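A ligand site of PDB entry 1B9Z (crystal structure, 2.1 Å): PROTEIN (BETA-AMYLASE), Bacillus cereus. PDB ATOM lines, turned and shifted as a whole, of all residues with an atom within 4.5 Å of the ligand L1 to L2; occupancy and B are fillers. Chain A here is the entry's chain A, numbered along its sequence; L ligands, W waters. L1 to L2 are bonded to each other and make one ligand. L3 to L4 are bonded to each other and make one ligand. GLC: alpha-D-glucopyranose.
The side-chain hydroxyl (OG1) of Thr 330 is in hydrogen-bond range of an oxygen (O3) of GLC L4 (2.7 Å). The backbone carbonyl oxygen (O) of Thr 330 sits at hydrogen-bond distance from an oxygen (O1) of GLC L1, at 3.3 Å. An oxygen (O6) of GLC L1 is in hydrogen-bond range of the side-chain carboxylate of Glu 367 (3.1 Å). NZ of Lys 287 sits at hydrogen-bond distance from O6 of GLC L1 (3.0 Å). NE2 of His 89 sits at hydrogen-bond distance from O3 of GLC L2. An oxygen (O2) of GLC L2 lies within hydrogen-bond range of the side-chain carboxylate (OD1) of Asp 97. The guanidinium group of Arg 397 is in hydrogen-bond range of an oxygen (O6) of GLC L2 (2.9 Å). An oxygen (O4) of GLC L4 sits at hydrogen-bond distance from the side-chain carboxylate (OE2) of Glu 172, at 2.6 Å. O of Val 95 lies within hydrogen-bond range of O3 of GLC L1 (3.3 Å). The side-chain carboxylate (OD2) of Asp 49 lies within hydrogen-bond range of an oxygen (O4) of GLC L2. An oxygen (O2) of GLC L1 is in hydrogen-bond range of the backbone carbonyl oxygen (O) of Ala 369 (2.7 Å). The side-chain hydroxyl (OG1) of Thr 330 sits at hydrogen-bond distance from an oxygen (O1) of GLC L1, at 2.9 Å.
O3 of GLC L4 lies within hydrogen-bond range of O1 of GLC L1 (2.8 Å).
The backbone carbonyl oxygen (O) of Leu 19 sits at hydrogen-bond distance from the indole nitrogen (NE1) of Trp 51, 3.4 Å away. OG1 of Thr 330 is in hydrogen-bond range of OE2 of Glu 172, at 3.1 Å. OD2 of Asp 97 sits at hydrogen-bond distance from N of Asn 94, 3.3 Å away. The side-chain carboxylate (OD2) of Asp 49 lies within hydrogen-bond range of the side-chain hydroxyl (OG) of Ser 87, at 2.7 Å. The side-chain carboxylate of Glu 367 lies within salt-bridge range of the side-chain amino group of Lys 287.
O5 of GLC L1 sits close to OE2 of Glu 172 (3.2 Å). Met 16 touches the ligand L1 to L2. Trp 51 touches the ligand L1 to L2. O of Ala 170 touches C6 of GLC L1, at 3.2 Å. CD2 of Leu 396 touches O3 of GLC L1, 3.7 Å away. Within 4 Å of the ligand L1 to L2: Met 16, Asp 49, Trp 51, His 89, Val 95, Asp 97, Ala 170, Glu 172, Lys 287, Thr 330, Glu 367, Ala 369, Leu 396 and Arg 397. The nearest printed residue that does not touch the ligand L1 to L2 is Leu 19 (4.02 Å).
Water W7 bridges O2 of GLC L2 and O of Val 95. Water W1 lies within hydrogen-bond range of the backbone carbonyl oxygen (O) of Val 95, an oxygen (O3) of GLC L1 and the side-chain carboxylate (OD1) of Asp 97. Water W5 lies within hydrogen-bond range of the side-chain carboxylate (OE1) of Glu 367 (2.7 Å), an oxygen (O1) of GLC L1 (2.9 Å) and the backbone carbonyl oxygen (O) of Thr 330 (3.2 Å). Water W3 lies within hydrogen-bond range of the side-chain amino group (NZ) of Lys 287 (2.8 Å) and an oxygen (O4) of GLC L2 (3.0 Å). Water W2 lies within hydrogen-bond range of the backbone carbonyl oxygen of Ala 369 (2.9 Å), an oxygen (O3) of GLC L1 (3.1 Å) and the backbone carbonyl oxygen of Val 95 (3.3 Å).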
ATOM      1  N   MET A  16       1.428  14.048  -0.586  1.00  0.00           N
ATOM      2  CA  MET A  16       1.598  12.669  -0.157  1.00  0.00           C
ATOM      3  C   MET A  16       1.934  12.710   1.331  1.00  0.00           C
ATOM      4  O   MET A  16       2.718  13.549   1.787  1.00  0.00           O
ATOM      5  CB  MET A  16       2.757  12.001  -0.869  1.00  0.00           C
ATOM      6  CG  MET A  16       2.365  11.236  -2.113  1.00  0.00           C
ATOM      7  SD  MET A  16       3.818  10.436  -2.869  1.00  0.00           S
ATOM      8  CE  MET A  16       3.751  11.098  -4.506  1.00  0.00           C
ATOM      9  N   LEU A  19       5.415   7.711   4.802  1.00  0.00           N
ATOM     10  CA  LEU A  19       5.238   6.285   4.557  1.00  0.00           C
ATOM     11  C   LEU A  19       4.842   5.574   5.888  1.00  0.00           C
ATOM     12  O   LEU A  19       4.113   4.579   5.981  1.00  0.00           O
ATOM     13  CB  LEU A  19       6.541   5.726   3.980  1.00  0.00           C
ATOM     14  CG  LEU A  19       6.895   6.123   2.546  1.00  0.00           C
ATOM     15  CD1 LEU A  19       8.213   5.534   2.226  1.00  0.00           C
ATOM     16  CD2 LEU A  19       5.885   5.583   1.510  1.00  0.00           C
ATOM     17  N   ASP A  49      -0.956   5.861   2.116  1.00  0.00           N
ATOM     18  CA  ASP A  49      -0.925   4.436   1.936  1.00  0.00           C
ATOM     19  C   ASP A  49      -1.531   3.700   3.136  1.00  0.00           C
ATOM     20  O   ASP A  49      -1.188   4.019   4.279  1.00  0.00           O
ATOM     21  CB  ASP A  49       0.468   3.840   1.855  1.00  0.00           C
ATOM     22  CG  ASP A  49       1.229   4.240   0.649  1.00  0.00           C
ATOM     23  OD1 ASP A  49       1.828   5.290   0.717  1.00  0.00           O
ATOM     24  OD2 ASP A  49       1.227   3.526  -0.351  1.00  0.00           O
ATOM     25  N   TRP A  51      -1.375   0.042   4.207  1.00  0.00           N
ATOM     26  CA  TRP A  51      -0.680  -1.187   3.855  1.00  0.00           C
ATOM     27  C   TRP A  51      -1.447  -2.470   4.118  1.00  0.00           C
ATOM     28  O   TRP A  51      -2.196  -2.554   5.099  1.00  0.00           O
ATOM     29  CB  TRP A  51       0.686  -1.281   4.608  1.00  0.00           C
ATOM     30  CG  TRP A  51       1.584  -0.068   4.350  1.00  0.00           C
ATOM     31  CD1 TRP A  51       1.729   0.956   5.266  1.00  0.00           C
ATOM     32  CD2 TRP A  51       2.231   0.196   3.183  1.00  0.00           C
ATOM     33  NE1 TRP A  51       2.447   1.868   4.677  1.00  0.00           N
ATOM     34  CE2 TRP A  51       2.762   1.477   3.429  1.00  0.00           C
ATOM     35  CE3 TRP A  51       2.432  -0.439   1.951  1.00  0.00           C
ATOM     36  CZ2 TRP A  51       3.509   2.116   2.418  1.00  0.00           C
ATOM     37  CZ3 TRP A  51       3.166   0.192   0.969  1.00  0.00           C
ATOM     38  CH2 TRP A  51       3.701   1.461   1.197  1.00  0.00           C
ATOM     39  N   ILE A  85      -4.781   4.811  -0.652  1.00  0.00           N
ATOM     40  CA  ILE A  85      -4.103   3.960  -1.616  1.00  0.00           C
ATOM     41  C   ILE A  85      -4.220   2.563  -0.957  1.00  0.00           C
ATOM     42  O   ILE A  85      -3.754   2.369   0.180  1.00  0.00           O
ATOM     43  CB  ILE A  85      -2.625   4.336  -1.773  1.00  0.00           C
ATOM     44  CG1 ILE A  85      -2.507   5.778  -2.257  1.00  0.00           C
ATOM     45  CG2 ILE A  85      -1.927   3.360  -2.745  1.00  0.00           C
ATOM     46  CD1 ILE A  85      -1.040   6.281  -2.228  1.00  0.00           C
ATOM     47  N   SER A  87      -2.717  -0.270  -0.662  1.00  0.00           N
ATOM     48  CA  SER A  87      -1.396  -0.792  -0.949  1.00  0.00           C
ATOM     49  C   SER A  87      -1.130  -2.240  -0.673  1.00  0.00           C
ATOM     50  O   SER A  87      -0.701  -2.633   0.406  1.00  0.00           O
ATOM     51  CB  SER A  87      -0.361   0.017  -0.213  1.00  0.00           C
ATOM     52  OG  SER A  87      -0.428   1.391  -0.539  1.00  0.00           O
ATOM     53  N   HIS A  89       1.287  -3.886  -1.952  1.00  0.00           N
ATOM     54  CA  HIS A  89       2.701  -4.104  -2.221  1.00  0.00           C
ATOM     55  C   HIS A  89       3.505  -3.820  -0.928  1.00  0.00           C
ATOM     56  O   HIS A  89       2.997  -3.186   0.001  1.00  0.00           O
ATOM     57  CB  HIS A  89       3.251  -3.144  -3.327  1.00  0.00           C
ATOM     58  CG  HIS A  89       3.059  -1.653  -2.994  1.00  0.00           C
ATOM     59  ND1 HIS A  89       1.962  -0.915  -3.178  1.00  0.00           N
ATOM     60  CD2 HIS A  89       4.015  -0.812  -2.481  1.00  0.00           C
ATOM     61  CE1 HIS A  89       2.191   0.326  -2.807  1.00  0.00           C
ATOM     62  NE2 HIS A  89       3.428   0.371  -2.396  1.00  0.00           N
ATOM     63  N   GLN A  90       4.784  -4.225  -0.916  1.00  0.00           N
ATOM     64  CA  GLN A  90       5.672  -4.020   0.185  1.00  0.00           C
ATOM     65  C   GLN A  90       6.214  -2.604   0.327  1.00  0.00           C
ATOM     66  O   GLN A  90       6.462  -1.932  -0.658  1.00  0.00           O
ATOM     67  CB  GLN A  90       6.813  -4.967   0.022  1.00  0.00           C
ATOM     68  CG  GLN A  90       7.879  -4.848   1.088  1.00  0.00           C
ATOM     69  CD  GLN A  90       8.886  -5.969   1.053  1.00  0.00           C
ATOM     70  OE1 GLN A  90       8.545  -7.144   1.059  1.00  0.00           O
ATOM     71  NE2 GLN A  90      10.156  -5.639   1.026  1.00  0.00           N
ATOM     72  N   ASN A  94      12.472   0.162  -2.078  1.00  0.00           N
ATOM     73  CA  ASN A  94      12.530   1.094  -3.200  1.00  0.00           C
ATOM     74  C   ASN A  94      13.054   2.496  -2.822  1.00  0.00           C
ATOM     75  O   ASN A  94      13.309   2.773  -1.648  1.00  0.00           O
ATOM     76  CB  ASN A  94      11.122   1.157  -3.806  1.00  0.00           C
ATOM     77  CG  ASN A  94      10.768  -0.209  -4.379  1.00  0.00           C
ATOM     78  OD1 ASN A  94       9.716  -0.785  -4.134  1.00  0.00           O
ATOM     79  ND2 ASN A  94      11.615  -0.825  -5.176  1.00  0.00           N
ATOM     80  N   VAL A  95      13.264   3.396  -3.819  1.00  0.00           N
ATOM     81  CA  VAL A  95      13.767   4.770  -3.631  1.00  0.00           C
ATOM     82  C   VAL A  95      12.861   5.657  -2.786  1.00  0.00           C
ATOM     83  O   VAL A  95      11.702   5.967  -3.117  1.00  0.00           O
ATOM     84  CB  VAL A  95      14.047   5.520  -5.067  1.00  0.00           C
ATOM     85  CG1 VAL A  95      12.819   5.546  -6.008  1.00  0.00           C
ATOM     86  CG2 VAL A  95      14.423   6.998  -4.808  1.00  0.00           C
ATOM     87  N   ASP A  97      11.976   4.954   0.372  1.00  0.00           N
ATOM     88  CA  ASP A  97      11.303   4.206   1.423  1.00  0.00           C
ATOM     89  C   ASP A  97      12.137   4.151   2.668  1.00  0.00           C
ATOM     90  O   ASP A  97      13.354   3.927   2.688  1.00  0.00           O
ATOM     91  CB  ASP A  97      10.971   2.755   1.032  1.00  0.00           C
ATOM     92  CG  ASP A  97      10.036   2.511  -0.155  1.00  0.00           C
ATOM     93  OD1 ASP A  97       9.562   3.477  -0.749  1.00  0.00           O
ATOM     94  OD2 ASP A  97       9.785   1.355  -0.499  1.00  0.00           O
ATOM     95  N   ALA A 170       6.103  -0.766  -5.509  1.00  0.00           N
ATOM     96  CA  ALA A 170       5.994   0.679  -5.260  1.00  0.00           C
ATOM     97  C   ALA A 170       4.667   1.289  -5.690  1.00  0.00           C
ATOM     98  O   ALA A 170       4.569   2.485  -5.935  1.00  0.00           O
ATOM     99  CB  ALA A 170       7.100   1.482  -5.976  1.00  0.00           C
ATOM    100  N   GLU A 172       2.938   0.701  -8.521  1.00  0.00           N
ATOM    101  CA  GLU A 172       2.828   0.949  -9.964  1.00  0.00           C
ATOM    102  C   GLU A 172       2.547  -0.305 -10.775  1.00  0.00           C
ATOM    103  O   GLU A 172       3.000  -1.384 -10.388  1.00  0.00           O
ATOM    104  CB  GLU A 172       4.151   1.595 -10.459  1.00  0.00           C
ATOM    105  CG  GLU A 172       4.394   2.924  -9.777  1.00  0.00           C
ATOM    106  CD  GLU A 172       5.802   3.470  -9.824  1.00  0.00           C
ATOM    107  OE1 GLU A 172       6.769   2.709  -9.612  1.00  0.00           O
ATOM    108  OE2 GLU A 172       5.894   4.686 -10.041  1.00  0.00           O
ATOM    109  N   LYS A 287      -1.266   3.632 -11.175  1.00  0.00           N
ATOM    110  CA  LYS A 287      -0.102   4.407 -11.611  1.00  0.00           C
ATOM    111  C   LYS A 287       0.874   3.636 -12.479  1.00  0.00           C
ATOM    112  O   LYS A 287       1.051   2.418 -12.371  1.00  0.00           O
ATOM    113  CB  LYS A 287       0.705   4.917 -10.412  1.00  0.00           C
ATOM    114  CG  LYS A 287      -0.071   5.459  -9.260  1.00  0.00           C
ATOM    115  CD  LYS A 287       0.881   5.746  -8.107  1.00  0.00           C
ATOM    116  CE  LYS A 287       0.071   6.444  -6.996  1.00  0.00           C
ATOM    117  NZ  LYS A 287       1.013   6.860  -5.969  1.00  0.00           N
ATOM    118  N   THR A 330       4.241   9.099 -12.854  1.00  0.00           N
ATOM    119  CA  THR A 330       5.040   9.569 -11.754  1.00  0.00           C
ATOM    120  C   THR A 330       6.377  10.247 -11.983  1.00  0.00           C
ATOM    121  O   THR A 330       7.185  10.140 -11.053  1.00  0.00           O
ATOM    122  CB  THR A 330       5.192   8.339 -10.733  1.00  0.00           C
ATOM    123  OG1 THR A 330       6.238   7.531 -11.243  1.00  0.00           O
ATOM    124  CG2 THR A 330       3.956   7.461 -10.567  1.00  0.00           C
ATOM    125  N   GLU A 367       2.984  13.381 -10.757  1.00  0.00           N
ATOM    126  CA  GLU A 367       3.741  13.305  -9.491  1.00  0.00           C
ATOM    127  C   GLU A 367       5.224  13.559  -9.757  1.00  0.00           C
ATOM    128  O   GLU A 367       5.733  13.404 -10.872  1.00  0.00           O
ATOM    129  CB  GLU A 367       3.785  11.953  -8.836  1.00  0.00           C
ATOM    130  CG  GLU A 367       2.491  11.331  -8.457  1.00  0.00           C
ATOM    131  CD  GLU A 367       2.674   9.969  -7.818  1.00  0.00           C
ATOM    132  OE1 GLU A 367       3.775   9.397  -7.819  1.00  0.00           O
ATOM    133  OE2 GLU A 367       1.697   9.465  -7.283  1.00  0.00           O
ATOM    134  N   ALA A 369       9.105  12.407  -9.169  1.00  0.00           N
ATOM    135  CA  ALA A 369       9.736  11.139  -8.795  1.00  0.00           C
ATOM    136  C   ALA A 369      10.583  11.209  -7.524  1.00  0.00           C
ATOM    137  O   ALA A 369      10.669  10.242  -6.746  1.00  0.00           O
ATOM    138  CB  ALA A 369      10.608  10.643  -9.964  1.00  0.00           C
ATOM    139  N   LEU A 396       5.410  14.678  -3.604  1.00  0.00           N
ATOM    140  CA  LEU A 396       6.123  13.681  -2.819  1.00  0.00           C
ATOM    141  C   LEU A 396       7.085  14.636  -2.120  1.00  0.00           C
ATOM    142  O   LEU A 396       7.927  15.226  -2.803  1.00  0.00           O
ATOM    143  CB  LEU A 396       6.874  12.720  -3.742  1.00  0.00           C
ATOM    144  CG  LEU A 396       8.105  11.762  -3.566  1.00  0.00           C
ATOM    145  CD1 LEU A 396       9.146  12.149  -2.503  1.00  0.00           C
ATOM    146  CD2 LEU A 396       7.516  10.434  -3.290  1.00  0.00           C
ATOM    147  N   ARG A 397       7.164  14.866  -0.799  1.00  0.00           N
ATOM    148  CA  ARG A 397       6.343  14.241   0.227  1.00  0.00           C
ATOM    149  C   ARG A 397       6.199  15.207   1.394  1.00  0.00           C
ATOM    150  O   ARG A 397       6.971  16.144   1.464  1.00  0.00           O
ATOM    151  CB  ARG A 397       7.088  12.982   0.579  1.00  0.00           C
ATOM    152  CG  ARG A 397       6.699  12.122   1.726  1.00  0.00           C
ATOM    153  CD  ARG A 397       7.450  10.820   1.501  1.00  0.00           C
ATOM    154  NE  ARG A 397       6.336   9.994   1.351  1.00  0.00           N
ATOM    155  CZ  ARG A 397       6.064   9.113   0.428  1.00  0.00           C
ATOM    156  NH1 ARG A 397       6.806   8.738  -0.606  1.00  0.00           N
ATOM    157  NH2 ARG A 397       4.806   8.704   0.571  1.00  0.00           N
HETATM  158  C1  GLC L   1       7.885   6.905  -7.877  1.00  0.00           C
HETATM  159  C2  GLC L   1       8.600   7.494  -6.686  1.00  0.00           C
HETATM  160  C3  GLC L   1       8.403   6.555  -5.523  1.00  0.00           C
HETATM  161  C4  GLC L   1       6.906   6.228  -5.283  1.00  0.00           C
HETATM  162  C5  GLC L   1       6.180   5.767  -6.600  1.00  0.00           C
HETATM  163  C6  GLC L   1       4.649   5.635  -6.560  1.00  0.00           C
HETATM  164  O1  GLC L   1       8.053   7.699  -9.024  1.00  0.00           O
HETATM  165  O2  GLC L   1       9.977   7.668  -6.980  1.00  0.00           O
HETATM  166  O3  GLC L   1       8.930   7.135  -4.351  1.00  0.00           O
HETATM  167  O4  GLC L   1       6.845   5.141  -4.338  1.00  0.00           O
HETATM  168  O5  GLC L   1       6.471   6.705  -7.644  1.00  0.00           O
HETATM  169  O6  GLC L   1       3.991   6.842  -6.160  1.00  0.00           O
HETATM  170  C1  GLC L   2       6.719   5.436  -2.968  1.00  0.00           C
HETATM  171  C2  GLC L   2       6.757   4.109  -2.275  1.00  0.00           C
HETATM  172  C3  GLC L   2       5.468   3.354  -2.535  1.00  0.00           C
HETATM  173  C4  GLC L   2       4.270   4.174  -2.109  1.00  0.00           C
HETATM  174  C5  GLC L   2       4.232   5.460  -2.850  1.00  0.00           C
HETATM  175  C6  GLC L   2       3.068   6.386  -2.452  1.00  0.00           C
HETATM  176  O2  GLC L   2       7.847   3.373  -2.743  1.00  0.00           O
HETATM  177  O3  GLC L   2       5.479   2.137  -1.800  1.00  0.00           O
HETATM  178  O4  GLC L   2       3.084   3.446  -2.377  1.00  0.00           O
HETATM  179  O5  GLC L   2       5.497   6.155  -2.648  1.00  0.00           O
HETATM  180  O6  GLC L   2       3.241   6.968  -1.181  1.00  0.00           O
HETATM  181  C1  GLC L   3      17.086   7.362  -9.897  1.00  0.00           C
HETATM  182  C2  GLC L   3      16.281   8.174 -10.958  1.00  0.00           C
HETATM  183  C3  GLC L   3      14.803   8.133 -10.574  1.00  0.00           C
HETATM  184  C4  GLC L   3      14.386   6.675 -10.339  1.00  0.00           C
HETATM  185  C5  GLC L   3      15.181   6.057  -9.200  1.00  0.00           C
HETATM  186  C6  GLC L   3      14.789   4.637  -8.705  1.00  0.00           C
HETATM  187  O1  GLC L   3      17.273   8.042  -8.675  1.00  0.00           O
HETATM  188  O2  GLC L   3      16.729   9.526 -11.072  1.00  0.00           O
HETATM  189  O3  GLC L   3      14.021   8.709 -11.593  1.00  0.00           O
HETATM  190  O4  GLC L   3      12.979   6.572 -10.042  1.00  0.00           O
HETATM  191  O5  GLC L   3      16.535   6.061  -9.642  1.00  0.00           O
HETATM  192  O6  GLC L   3      15.159   3.650  -9.608  1.00  0.00           O
HETATM  193  C1  GLC L   4      12.337   5.596 -10.877  1.00  0.00           C
HETATM  194  C2  GLC L   4      11.180   6.217 -11.738  1.00  0.00           C
HETATM  195  C3  GLC L   4       9.909   6.268 -10.870  1.00  0.00           C
HETATM  196  C4  GLC L   4       9.726   4.854 -10.346  1.00  0.00           C
HETATM  197  C5  GLC L   4      10.818   4.597  -9.300  1.00  0.00           C
HETATM  198  C6  GLC L   4      10.620   3.403  -8.312  1.00  0.00           C
HETATM  199  O2  GLC L   4      11.499   7.515 -12.233  1.00  0.00           O
HETATM  200  O3  GLC L   4       8.758   6.720 -11.563  1.00  0.00           O
HETATM  201  O4  GLC L   4       8.478   4.707  -9.804  1.00  0.00           O
HETATM  202  O5  GLC L   4      11.999   4.447 -10.078  1.00  0.00           O
HETATM  203  O6  GLC L   4       9.452   2.680  -8.618  1.00  0.00           O
HETATM  204  O   HOH W   1       9.382   6.454  -1.590  1.00  0.00           O
HETATM  205  O   HOH W   2      11.329   9.077  -4.219  1.00  0.00           O
HETATM  206  O   HOH W   3       1.714   4.395  -4.857  1.00  0.00           O
HETATM  207  O   HOH W   4       7.691   0.419  -1.844  1.00  0.00           O
HETATM  208  O   HOH W   5       6.402   9.892  -7.998  1.00  0.00           O
HETATM  209  O   HOH W   6       1.074   9.009  -0.364  1.00  0.00           O
HETATM  210  O   HOH W   7       9.820   4.135  -4.418  1.00  0.00           O
